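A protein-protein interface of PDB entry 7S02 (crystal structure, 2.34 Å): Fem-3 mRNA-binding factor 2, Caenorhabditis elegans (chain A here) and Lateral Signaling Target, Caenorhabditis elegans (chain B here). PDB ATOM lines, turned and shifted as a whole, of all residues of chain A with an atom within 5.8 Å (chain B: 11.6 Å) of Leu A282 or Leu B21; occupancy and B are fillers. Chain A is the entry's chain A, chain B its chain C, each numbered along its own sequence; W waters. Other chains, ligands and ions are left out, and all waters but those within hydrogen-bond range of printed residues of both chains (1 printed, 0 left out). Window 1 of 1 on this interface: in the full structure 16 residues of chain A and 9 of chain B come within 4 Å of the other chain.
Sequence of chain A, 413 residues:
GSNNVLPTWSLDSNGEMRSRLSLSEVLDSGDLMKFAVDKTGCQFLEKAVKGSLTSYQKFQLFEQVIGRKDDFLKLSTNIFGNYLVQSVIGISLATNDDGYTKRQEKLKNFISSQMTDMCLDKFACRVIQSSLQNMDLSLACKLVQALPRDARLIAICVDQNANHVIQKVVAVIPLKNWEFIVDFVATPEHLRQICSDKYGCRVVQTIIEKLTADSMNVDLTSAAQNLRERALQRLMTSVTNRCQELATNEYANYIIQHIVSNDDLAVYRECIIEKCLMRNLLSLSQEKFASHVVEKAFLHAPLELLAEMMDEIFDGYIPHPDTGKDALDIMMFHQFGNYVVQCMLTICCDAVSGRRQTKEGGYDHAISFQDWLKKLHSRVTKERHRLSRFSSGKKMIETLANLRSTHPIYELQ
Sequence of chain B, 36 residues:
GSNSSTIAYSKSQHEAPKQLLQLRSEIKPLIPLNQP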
ATOM      1  N   ASN A 280     -22.964  19.575   6.028  1.00  0.00           N
ATOM      2  CA  ASN A 280     -21.982  19.586   4.951  1.00  0.00           C
ATOM      3  C   ASN A 280     -22.649  19.644   3.579  1.00  0.00           C
ATOM      4  O   ASN A 280     -22.002  19.334   2.573  1.00  0.00           O
ATOM      5  CB  ASN A 280     -21.068  18.353   5.015  1.00  0.00           C
ATOM      6  CG  ASN A 280     -20.257  18.290   6.296  1.00  0.00           C
ATOM      7  OD1 ASN A 280     -20.705  17.739   7.302  1.00  0.00           O
ATOM      8  ND2 ASN A 280     -19.053  18.852   6.263  1.00  0.00           N
ATOM      9  N   LEU A 281     -23.924  20.038   3.517  1.00  0.00           N
ATOM     10  CA  LEU A 281     -24.665  19.965   2.261  1.00  0.00           C
ATOM     11  C   LEU A 281     -24.100  20.923   1.219  1.00  0.00           C
ATOM     12  O   LEU A 281     -23.956  20.558   0.048  1.00  0.00           O
ATOM     13  CB  LEU A 281     -26.144  20.255   2.512  1.00  0.00           C
ATOM     14  CG  LEU A 281     -26.877  19.265   3.422  1.00  0.00           C
ATOM     15  CD1 LEU A 281     -28.354  19.612   3.523  1.00  0.00           C
ATOM     16  CD2 LEU A 281     -26.693  17.842   2.917  1.00  0.00           C
ATOM     17  N   LEU A 282     -23.771  22.152   1.625  1.00  0.00           N
ATOM     18  CA  LEU A 282     -23.266  23.133   0.670  1.00  0.00           C
ATOM     19  C   LEU A 282     -21.914  22.715   0.103  1.00  0.00           C
ATOM     20  O   LEU A 282     -21.671  22.850  -1.102  1.00  0.00           O
ATOM     21  CB  LEU A 282     -23.170  24.508   1.331  1.00  0.00           C
ATOM     22  CG  LEU A 282     -22.488  25.613   0.524  1.00  0.00           C
ATOM     23  CD1 LEU A 282     -23.257  25.889  -0.758  1.00  0.00           C
ATOM     24  CD2 LEU A 282     -22.360  26.882   1.355  1.00  0.00           C
ATOM     25  N   SER A 283     -21.023  22.204   0.954  1.00  0.00           N
ATOM     26  CA  SER A 283     -19.712  21.768   0.481  1.00  0.00           C
ATOM     27  C   SER A 283     -19.833  20.550  -0.425  1.00  0.00           C
ATOM     28  O   SER A 283     -19.246  20.508  -1.511  1.00  0.00           O
ATOM     29  CB  SER A 283     -18.799  21.466   1.669  1.00  0.00           C
ATOM     30  OG  SER A 283     -17.559  20.934   1.236  1.00  0.00           O
ATOM     31  N   LEU A 284     -20.599  19.545   0.007  1.00  0.00           N
ATOM     32  CA  LEU A 284     -20.718  18.317  -0.770  1.00  0.00           C
ATOM     33  C   LEU A 284     -21.492  18.539  -2.065  1.00  0.00           C
ATOM     34  O   LEU A 284     -21.249  17.839  -3.054  1.00  0.00           O
ATOM     35  CB  LEU A 284     -21.384  17.232   0.075  1.00  0.00           C
ATOM     36  CG  LEU A 284     -20.537  16.732   1.249  1.00  0.00           C
ATOM     37  CD1 LEU A 284     -21.254  15.636   2.012  1.00  0.00           C
ATOM     38  CD2 LEU A 284     -19.180  16.245   0.767  1.00  0.00           C
ATOM     39  N   SER A 285     -22.414  19.504  -2.085  1.00  0.00           N
ATOM     40  CA  SER A 285     -23.164  19.786  -3.304  1.00  0.00           C
ATOM     41  C   SER A 285     -22.277  20.337  -4.410  1.00  0.00           C
ATOM     42  O   SER A 285     -22.667  20.296  -5.582  1.00  0.00           O
ATOM     43  CB  SER A 285     -24.299  20.771  -3.017  1.00  0.00           C
ATOM     44  OG  SER A 285     -25.293  20.181  -2.196  1.00  0.00           O
ATOM     45  N   GLN A 286     -21.096  20.849  -4.068  1.00  0.00           N
ATOM     46  CA  GLN A 286     -20.170  21.411  -5.039  1.00  0.00           C
ATOM     47  C   GLN A 286     -19.098  20.417  -5.471  1.00  0.00           C
ATOM     48  O   GLN A 286     -18.108  20.820  -6.090  1.00  0.00           O
ATOM     49  CB  GLN A 286     -19.519  22.674  -4.469  1.00  0.00           C
ATOM     50  CG  GLN A 286     -20.474  23.856  -4.354  1.00  0.00           C
ATOM     51  CD  GLN A 286     -19.880  25.019  -3.582  1.00  0.00           C
ATOM     52  OE1 GLN A 286     -19.296  25.932  -4.166  1.00  0.00           O
ATOM     53  NE2 GLN A 286     -20.023  24.989  -2.262  1.00  0.00           N
ATOM     54  N   GLU A 312     -31.183  23.643   6.262  1.00  0.00           N
ATOM     55  CA  GLU A 312     -29.752  23.920   6.176  1.00  0.00           C
ATOM     56  C   GLU A 312     -29.418  24.711   4.917  1.00  0.00           C
ATOM     57  O   GLU A 312     -28.602  25.639   4.956  1.00  0.00           O
ATOM     58  CB  GLU A 312     -28.951  22.619   6.215  1.00  0.00           C
ATOM     59  CG  GLU A 312     -27.460  22.825   5.975  1.00  0.00           C
ATOM     60  CD  GLU A 312     -26.637  21.577   6.227  1.00  0.00           C
ATOM     61  OE1 GLU A 312     -27.102  20.694   6.976  1.00  0.00           O
ATOM     62  OE2 GLU A 312     -25.522  21.482   5.671  1.00  0.00           O
ATOM     63  N   ILE A 313     -30.038  24.362   3.789  1.00  0.00           N
ATOM     64  CA  ILE A 313     -29.793  25.107   2.560  1.00  0.00           C
ATOM     65  C   ILE A 313     -30.405  26.498   2.650  1.00  0.00           C
ATOM     66  O   ILE A 313     -29.797  27.490   2.229  1.00  0.00           O
ATOM     67  CB  ILE A 313     -30.332  24.329   1.346  1.00  0.00           C
ATOM     68  CG1 ILE A 313     -29.698  22.938   1.282  1.00  0.00           C
ATOM     69  CG2 ILE A 313     -30.083  25.105   0.059  1.00  0.00           C
ATOM     70  CD1 ILE A 313     -28.187  22.960   1.193  1.00  0.00           C
ATOM     71  N   TYR A 317     -26.553  28.573   6.632  1.00  0.00           N
ATOM     72  CA  TYR A 317     -25.246  29.160   6.385  1.00  0.00           C
ATOM     73  C   TYR A 317     -25.305  30.678   6.477  1.00  0.00           C
ATOM     74  O   TYR A 317     -26.309  31.304   6.122  1.00  0.00           O
ATOM     75  CB  TYR A 317     -24.707  28.747   5.011  1.00  0.00           C
ATOM     76  CG  TYR A 317     -24.460  27.263   4.885  1.00  0.00           C
ATOM     77  CD1 TYR A 317     -23.249  26.707   5.274  1.00  0.00           C
ATOM     78  CD2 TYR A 317     -25.440  26.417   4.384  1.00  0.00           C
ATOM     79  CE1 TYR A 317     -23.017  25.349   5.163  1.00  0.00           C
ATOM     80  CE2 TYR A 317     -25.218  25.057   4.270  1.00  0.00           C
ATOM     81  CZ  TYR A 317     -24.006  24.530   4.663  1.00  0.00           C
ATOM     82  OH  TYR A 317     -23.780  23.177   4.550  1.00  0.00           O
ATOM     83  N   ILE A 318     -24.215  31.258   6.960  1.00  0.00           N
ATOM     84  CA  ILE A 318     -24.086  32.716   7.017  1.00  0.00           C
ATOM     85  C   ILE A 318     -23.646  33.221   5.653  1.00  0.00           C
ATOM     86  O   ILE A 318     -22.654  32.713   5.101  1.00  0.00           O
ATOM     87  CB  ILE A 318     -23.094  33.121   8.105  1.00  0.00           C
ATOM     88  CG1 ILE A 318     -23.653  32.786   9.490  1.00  0.00           C
ATOM     89  CG2 ILE A 318     -22.768  34.604   8.002  1.00  0.00           C
ATOM     90  CD1 ILE A 318     -22.663  32.992  10.619  1.00  0.00           C
ATOM     91  N   PRO A 319     -24.344  34.195   5.065  1.00  0.00           N
ATOM     92  CA  PRO A 319     -23.970  34.678   3.732  1.00  0.00           C
ATOM     93  C   PRO A 319     -22.577  35.290   3.717  1.00  0.00           C
ATOM     94  O   PRO A 319     -21.993  35.609   4.754  1.00  0.00           O
ATOM     95  CB  PRO A 319     -25.041  35.728   3.412  1.00  0.00           C
ATOM     96  CG  PRO A 319     -26.178  35.423   4.323  1.00  0.00           C
ATOM     97  CD  PRO A 319     -25.590  34.809   5.556  1.00  0.00           C
ATOM     98  N   HIS A 320     -22.049  35.451   2.507  1.00  0.00           N
ATOM     99  CA  HIS A 320     -20.713  36.006   2.340  1.00  0.00           C
ATOM    100  C   HIS A 320     -20.684  37.441   2.853  1.00  0.00           C
ATOM    101  O   HIS A 320     -21.593  38.226   2.550  1.00  0.00           O
ATOM    102  CB  HIS A 320     -20.292  35.954   0.872  1.00  0.00           C
ATOM    103  CG  HIS A 320     -18.827  36.175   0.655  1.00  0.00           C
ATOM    104  ND1 HIS A 320     -18.253  37.427   0.663  1.00  0.00           N
ATOM    105  CD2 HIS A 320     -17.818  35.300   0.428  1.00  0.00           C
ATOM    106  CE1 HIS A 320     -16.955  37.316   0.448  1.00  0.00           C
ATOM    107  NE2 HIS A 320     -16.664  36.035   0.302  1.00  0.00           N
ATOM    108  N   LYS A 325     -23.980  36.670  -0.924  1.00  0.00           N
ATOM    109  CA  LYS A 325     -24.373  35.371  -1.453  1.00  0.00           C
ATOM    110  C   LYS A 325     -24.648  34.398  -0.315  1.00  0.00           C
ATOM    111  O   LYS A 325     -23.845  34.273   0.614  1.00  0.00           O
ATOM    112  CB  LYS A 325     -23.273  34.806  -2.350  1.00  0.00           C
ATOM    113  CG  LYS A 325     -23.128  35.471  -3.703  1.00  0.00           C
ATOM    114  CD  LYS A 325     -22.082  34.735  -4.526  1.00  0.00           C
ATOM    115  CE  LYS A 325     -22.019  35.242  -5.952  1.00  0.00           C
ATOM    116  NZ  LYS A 325     -21.068  34.435  -6.767  1.00  0.00           N
ATOM    117  N   ASP A 326     -25.777  33.702  -0.390  1.00  0.00           N
ATOM    118  CA  ASP A 326     -26.085  32.636   0.546  1.00  0.00           C
ATOM    119  C   ASP A 326     -25.876  31.286  -0.140  1.00  0.00           C
ATOM    120  O   ASP A 326     -25.335  31.203  -1.248  1.00  0.00           O
ATOM    121  CB  ASP A 326     -27.502  32.806   1.105  1.00  0.00           C
ATOM    122  CG  ASP A 326     -28.563  32.926   0.021  1.00  0.00           C
ATOM    123  OD1 ASP A 326     -28.373  32.385  -1.088  1.00  0.00           O
ATOM    124  OD2 ASP A 326     -29.603  33.565   0.287  1.00  0.00           O
ATOM    125  N   ALA A 327     -26.304  30.210   0.525  1.00  0.00           N
ATOM    126  CA  ALA A 327     -26.105  28.873  -0.026  1.00  0.00           C
ATOM    127  C   ALA A 327     -26.883  28.685  -1.323  1.00  0.00           C
ATOM    128  O   ALA A 327     -26.399  28.038  -2.258  1.00  0.00           O
ATOM    129  CB  ALA A 327     -26.509  27.816   1.000  1.00  0.00           C
ATOM    130  N   ILE A 330     -25.059  30.275  -4.253  1.00  0.00           N
ATOM    131  CA  ILE A 330     -23.876  29.540  -4.688  1.00  0.00           C
ATOM    132  C   ILE A 330     -24.276  28.302  -5.482  1.00  0.00           C
ATOM    133  O   ILE A 330     -23.768  28.061  -6.583  1.00  0.00           O
ATOM    134  CB  ILE A 330     -22.994  29.178  -3.480  1.00  0.00           C
ATOM    135  CG1 ILE A 330     -22.237  30.411  -2.983  1.00  0.00           C
ATOM    136  CG2 ILE A 330     -22.024  28.064  -3.841  1.00  0.00           C
ATOM    137  CD1 ILE A 330     -21.861  30.345  -1.524  1.00  0.00           C
ATOM    138  N   MET A 331     -25.195  27.500  -4.937  1.00  0.00           N
ATOM    139  CA  MET A 331     -25.547  26.242  -5.588  1.00  0.00           C
ATOM    140  C   MET A 331     -26.280  26.462  -6.904  1.00  0.00           C
ATOM    141  O   MET A 331     -26.096  25.684  -7.846  1.00  0.00           O
ATOM    142  CB  MET A 331     -26.400  25.382  -4.657  1.00  0.00           C
ATOM    143  CG  MET A 331     -25.644  24.759  -3.500  1.00  0.00           C
ATOM    144  SD  MET A 331     -26.670  24.663  -2.026  1.00  0.00           S
ATOM    145  CE  MET A 331     -27.621  23.192  -2.409  1.00  0.00           C
ATOM    146  N   PRO B  17     -13.306  24.856  -8.372  1.00  0.00           N
ATOM    147  CA  PRO B  17     -13.280  25.679  -7.162  1.00  0.00           C
ATOM    148  C   PRO B  17     -14.538  25.536  -6.308  1.00  0.00           C
ATOM    149  O   PRO B  17     -15.595  25.154  -6.811  1.00  0.00           O
ATOM    150  CB  PRO B  17     -13.150  27.100  -7.722  1.00  0.00           C
ATOM    151  CG  PRO B  17     -13.697  27.020  -9.150  1.00  0.00           C
ATOM    152  CD  PRO B  17     -13.954  25.570  -9.485  1.00  0.00           C
ATOM    153  N   LYS B  18     -14.413  25.841  -5.019  1.00  0.00           N
ATOM    154  CA  LYS B  18     -15.506  25.727  -4.065  1.00  0.00           C
ATOM    155  C   LYS B  18     -15.782  27.079  -3.426  1.00  0.00           C
ATOM    156  O   LYS B  18     -14.853  27.833  -3.120  1.00  0.00           O
ATOM    157  CB  LYS B  18     -15.185  24.706  -2.970  1.00  0.00           C
ATOM    158  CG  LYS B  18     -15.844  23.352  -3.147  1.00  0.00           C
ATOM    159  CD  LYS B  18     -15.588  22.475  -1.932  1.00  0.00           C
ATOM    160  CE  LYS B  18     -16.148  21.079  -2.123  1.00  0.00           C
ATOM    161  NZ  LYS B  18     -16.205  20.327  -0.838  1.00  0.00           N
ATOM    162  N   GLN B  19     -17.062  27.377  -3.222  1.00  0.00           N
ATOM    163  CA  GLN B  19     -17.495  28.563  -2.489  1.00  0.00           C
ATOM    164  C   GLN B  19     -18.130  28.085  -1.188  1.00  0.00           C
ATOM    165  O   GLN B  19     -19.282  27.643  -1.175  1.00  0.00           O
ATOM    166  CB  GLN B  19     -18.468  29.397  -3.316  1.00  0.00           C
ATOM    167  CG  GLN B  19     -17.820  30.546  -4.066  1.00  0.00           C
ATOM    168  CD  GLN B  19     -18.833  31.543  -4.589  1.00  0.00           C
ATOM    169  OE1 GLN B  19     -19.138  31.570  -5.781  1.00  0.00           O
ATOM    170  NE2 GLN B  19     -19.365  32.371  -3.696  1.00  0.00           N
ATOM    171  N   LEU B  20     -17.376  28.172  -0.099  1.00  0.00           N
ATOM    172  CA  LEU B  20     -17.826  27.698   1.201  1.00  0.00           C
ATOM    173  C   LEU B  20     -18.344  28.858   2.043  1.00  0.00           C
ATOM    174  O   LEU B  20     -17.867  29.991   1.939  1.00  0.00           O
ATOM    175  CB  LEU B  20     -16.693  26.983   1.941  1.00  0.00           C
ATOM    176  CG  LEU B  20     -16.238  25.646   1.349  1.00  0.00           C
ATOM    177  CD1 LEU B  20     -15.395  24.873   2.352  1.00  0.00           C
ATOM    178  CD2 LEU B  20     -17.432  24.820   0.897  1.00  0.00           C
ATOM    179  N   LEU B  21     -19.332  28.560   2.883  1.00  0.00           N
ATOM    180  CA  LEU B  21     -19.920  29.539   3.784  1.00  0.00           C
ATOM    181  C   LEU B  21     -19.858  29.019   5.212  1.00  0.00           C
ATOM    182  O   LEU B  21     -19.932  27.812   5.455  1.00  0.00           O
ATOM    183  CB  LEU B  21     -21.376  29.850   3.417  1.00  0.00           C
ATOM    184  CG  LEU B  21     -21.615  30.661   2.144  1.00  0.00           C
ATOM    185  CD1 LEU B  21     -23.107  30.787   1.878  1.00  0.00           C
ATOM    186  CD2 LEU B  21     -20.962  32.031   2.239  1.00  0.00           C
ATOM    187  N   GLN B  22     -19.725  29.947   6.155  1.00  0.00           N
ATOM    188  CA  GLN B  22     -19.688  29.577   7.562  1.00  0.00           C
ATOM    189  C   GLN B  22     -21.055  29.086   8.020  1.00  0.00           C
ATOM    190  O   GLN B  22     -22.092  29.642   7.649  1.00  0.00           O
ATOM    191  CB  GLN B  22     -19.244  30.766   8.411  1.00  0.00           C
ATOM    192  CG  GLN B  22     -18.607  30.381   9.735  1.00  0.00           C
ATOM    193  CD  GLN B  22     -18.264  31.588  10.583  1.00  0.00           C
ATOM    194  OE1 GLN B  22     -18.913  31.858  11.593  1.00  0.00           O
ATOM    195  NE2 GLN B  22     -17.237  32.325  10.174  1.00  0.00           N
ATOM    196  N   LEU B  23     -21.051  28.032   8.831  1.00  0.00           N
ATOM    197  CA  LEU B  23     -22.287  27.475   9.350  1.00  0.00           C
ATOM    198  C   LEU B  23     -22.799  28.301  10.525  1.00  0.00           C
ATOM    199  O   LEU B  23     -22.051  29.025  11.188  1.00  0.00           O
ATOM    200  CB  LEU B  23     -22.083  26.023   9.790  1.00  0.00           C
ATOM    201  CG  LEU B  23     -22.365  24.925   8.763  1.00  0.00           C
ATOM    202  CD1 LEU B  23     -21.470  23.721   9.013  1.00  0.00           C
ATOM    203  CD2 LEU B  23     -23.831  24.523   8.795  1.00  0.00           C
ATOM    204  N   ARG B  24     -24.100  28.183  10.777  1.00  0.00           N
ATOM    205  CA  ARG B  24     -24.709  28.774  11.955  1.00  0.00           C
ATOM    206  C   ARG B  24     -24.628  27.786  13.117  1.00  0.00           C
ATOM    207  O   ARG B  24     -24.136  26.664  12.979  1.00  0.00           O
ATOM    208  CB  ARG B  24     -26.153  29.181  11.664  1.00  0.00           C
ATOM    209  CG  ARG B  24     -26.288  30.542  11.001  1.00  0.00           C
ATOM    210  CD  ARG B  24     -27.725  31.040  11.024  1.00  0.00           C
ATOM    211  NE  ARG B  24     -28.691  29.949  10.980  1.00  0.00           N
ATOM    212  CZ  ARG B  24     -29.873  29.972  11.581  1.00  0.00           C
ATOM    213  NH1 ARG B  24     -30.270  31.020  12.285  1.00  0.00           N
ATOM    214  NH2 ARG B  24     -30.677  28.918  11.471  1.00  0.00           N
ATOM    215  N   SER B  25     -25.113  28.205  14.280  1.00  0.00           N
ATOM    216  CA  SER B  25     -25.098  27.353  15.457  1.00  0.00           C
ATOM    217  C   SER B  25     -26.361  26.497  15.516  1.00  0.00           C
ATOM    218  O   SER B  25     -27.333  26.720  14.791  1.00  0.00           O
ATOM    219  CB  SER B  25     -24.955  28.196  16.724  1.00  0.00           C
ATOM    220  OG  SER B  25     -23.646  28.726  16.838  1.00  0.00           O
HETATM  221  O   HOH W   1     -20.172  32.483   5.428  1.00  0.00           O
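Of chain B, only Leu B21 comes within 4 Å of Leu A282. No residue of chain B comes within 4 Å of Leu A281. Ser A283 touches just these residues of chain B: Lys B18 and Leu B20. No residue of chain B comes within 4 Å of Ser A285. Gln A286 touches just these residues of chain B: Lys B18 (3.8 Å) and Gln B19 (2.8 Å). Printed residues of chain B within 4 Å of Tyr A317: Leu B21 (3.5 Å), Gln B22 (3.4 Å) and Leu B23 (3.7 Å). Of the printed residues of chain B, His A320 touches Leu B21. Ala A327 touches just one residue of chain B: Leu B21. Printed residues of chain B within 4 Å of Lys A325: Gln B19 and Leu B21. Printed residues of chain A within 4 Å of Leu B20: Ser A283 (3.7 Å). Printed residues of chain A within 4 Å of Gln B22: Tyr A317 (3.4 Å) and Ile A318 (2.8 Å). The nearest printed residue of chain A that does not touch Leu B23 is Ile A318 (4.1 Å).
Among the printed residues, pairs that only touch across the chains: Ile A318 with Leu B21, Tyr A317 with Gln B22, Asp A326 with Leu B21, Tyr A317 with Leu B21, Ala A327 with Leu B21, Ile A330 with Gln B19, Lys A325 with Gln B19, His A320 with Leu B21, Ile A330 with Leu B21, Tyr A317 with Leu B23, Ser A283 with Leu B20, Leu A282 with Leu B21, Gln A286 with Lys B18, Ile A318 with Arg B24, Lys A325 with Leu B21 and Pro A319 with Leu B21.
The side-chain hydroxyl of Ser A283 is in hydrogen-bond range of the side-chain amino group of Lys B18 (2.6 Å). The side-chain amide oxygen (OE1) of Gln A286 sits at hydrogen-bond distance from the backbone NH (N) of Gln B19 (2.8 Å). The backbone NH of Ile A318 is in hydrogen-bond range of the backbone carbonyl oxygen of Gln B22, at 2.8 Å.
Hydrophobic or aromatic side chains of chain A that line the printed part of chain B: Leu A282, Tyr A317, Ile A318 and Ile A330. Among the printed residues, 19 pairs touch across the chains. Among the printed residues, no Asp or Glu carboxylate lies within 4 Å of a Lys or Arg side-chain nitrogen of the other chain.
The side-chain hydroxyl (OH) of Tyr A317 lies within hydrogen-bond range of the backbone NH (N) of Leu A281, at 3.3 Å. The backbone carbonyl oxygen (O) of Leu A282 is in hydrogen-bond range of the side-chain amide nitrogen (NE2) of Gln A286 (2.9 Å). The backbone NH of Leu A282 lies within hydrogen-bond range of the side-chain hydroxyl of Tyr A317 (3.1 Å). OH of Tyr A317 is in hydrogen-bond range of OE2 of Glu A312. The backbone carbonyl oxygen (O) of Lys A325 lies within hydrogen-bond range of the backbone NH (N) of His A320.
Water W1 bridges the backbone carbonyl oxygen of Ile A318 (2.5 Å) and the backbone NH of Gln B22 (2.7 Å).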
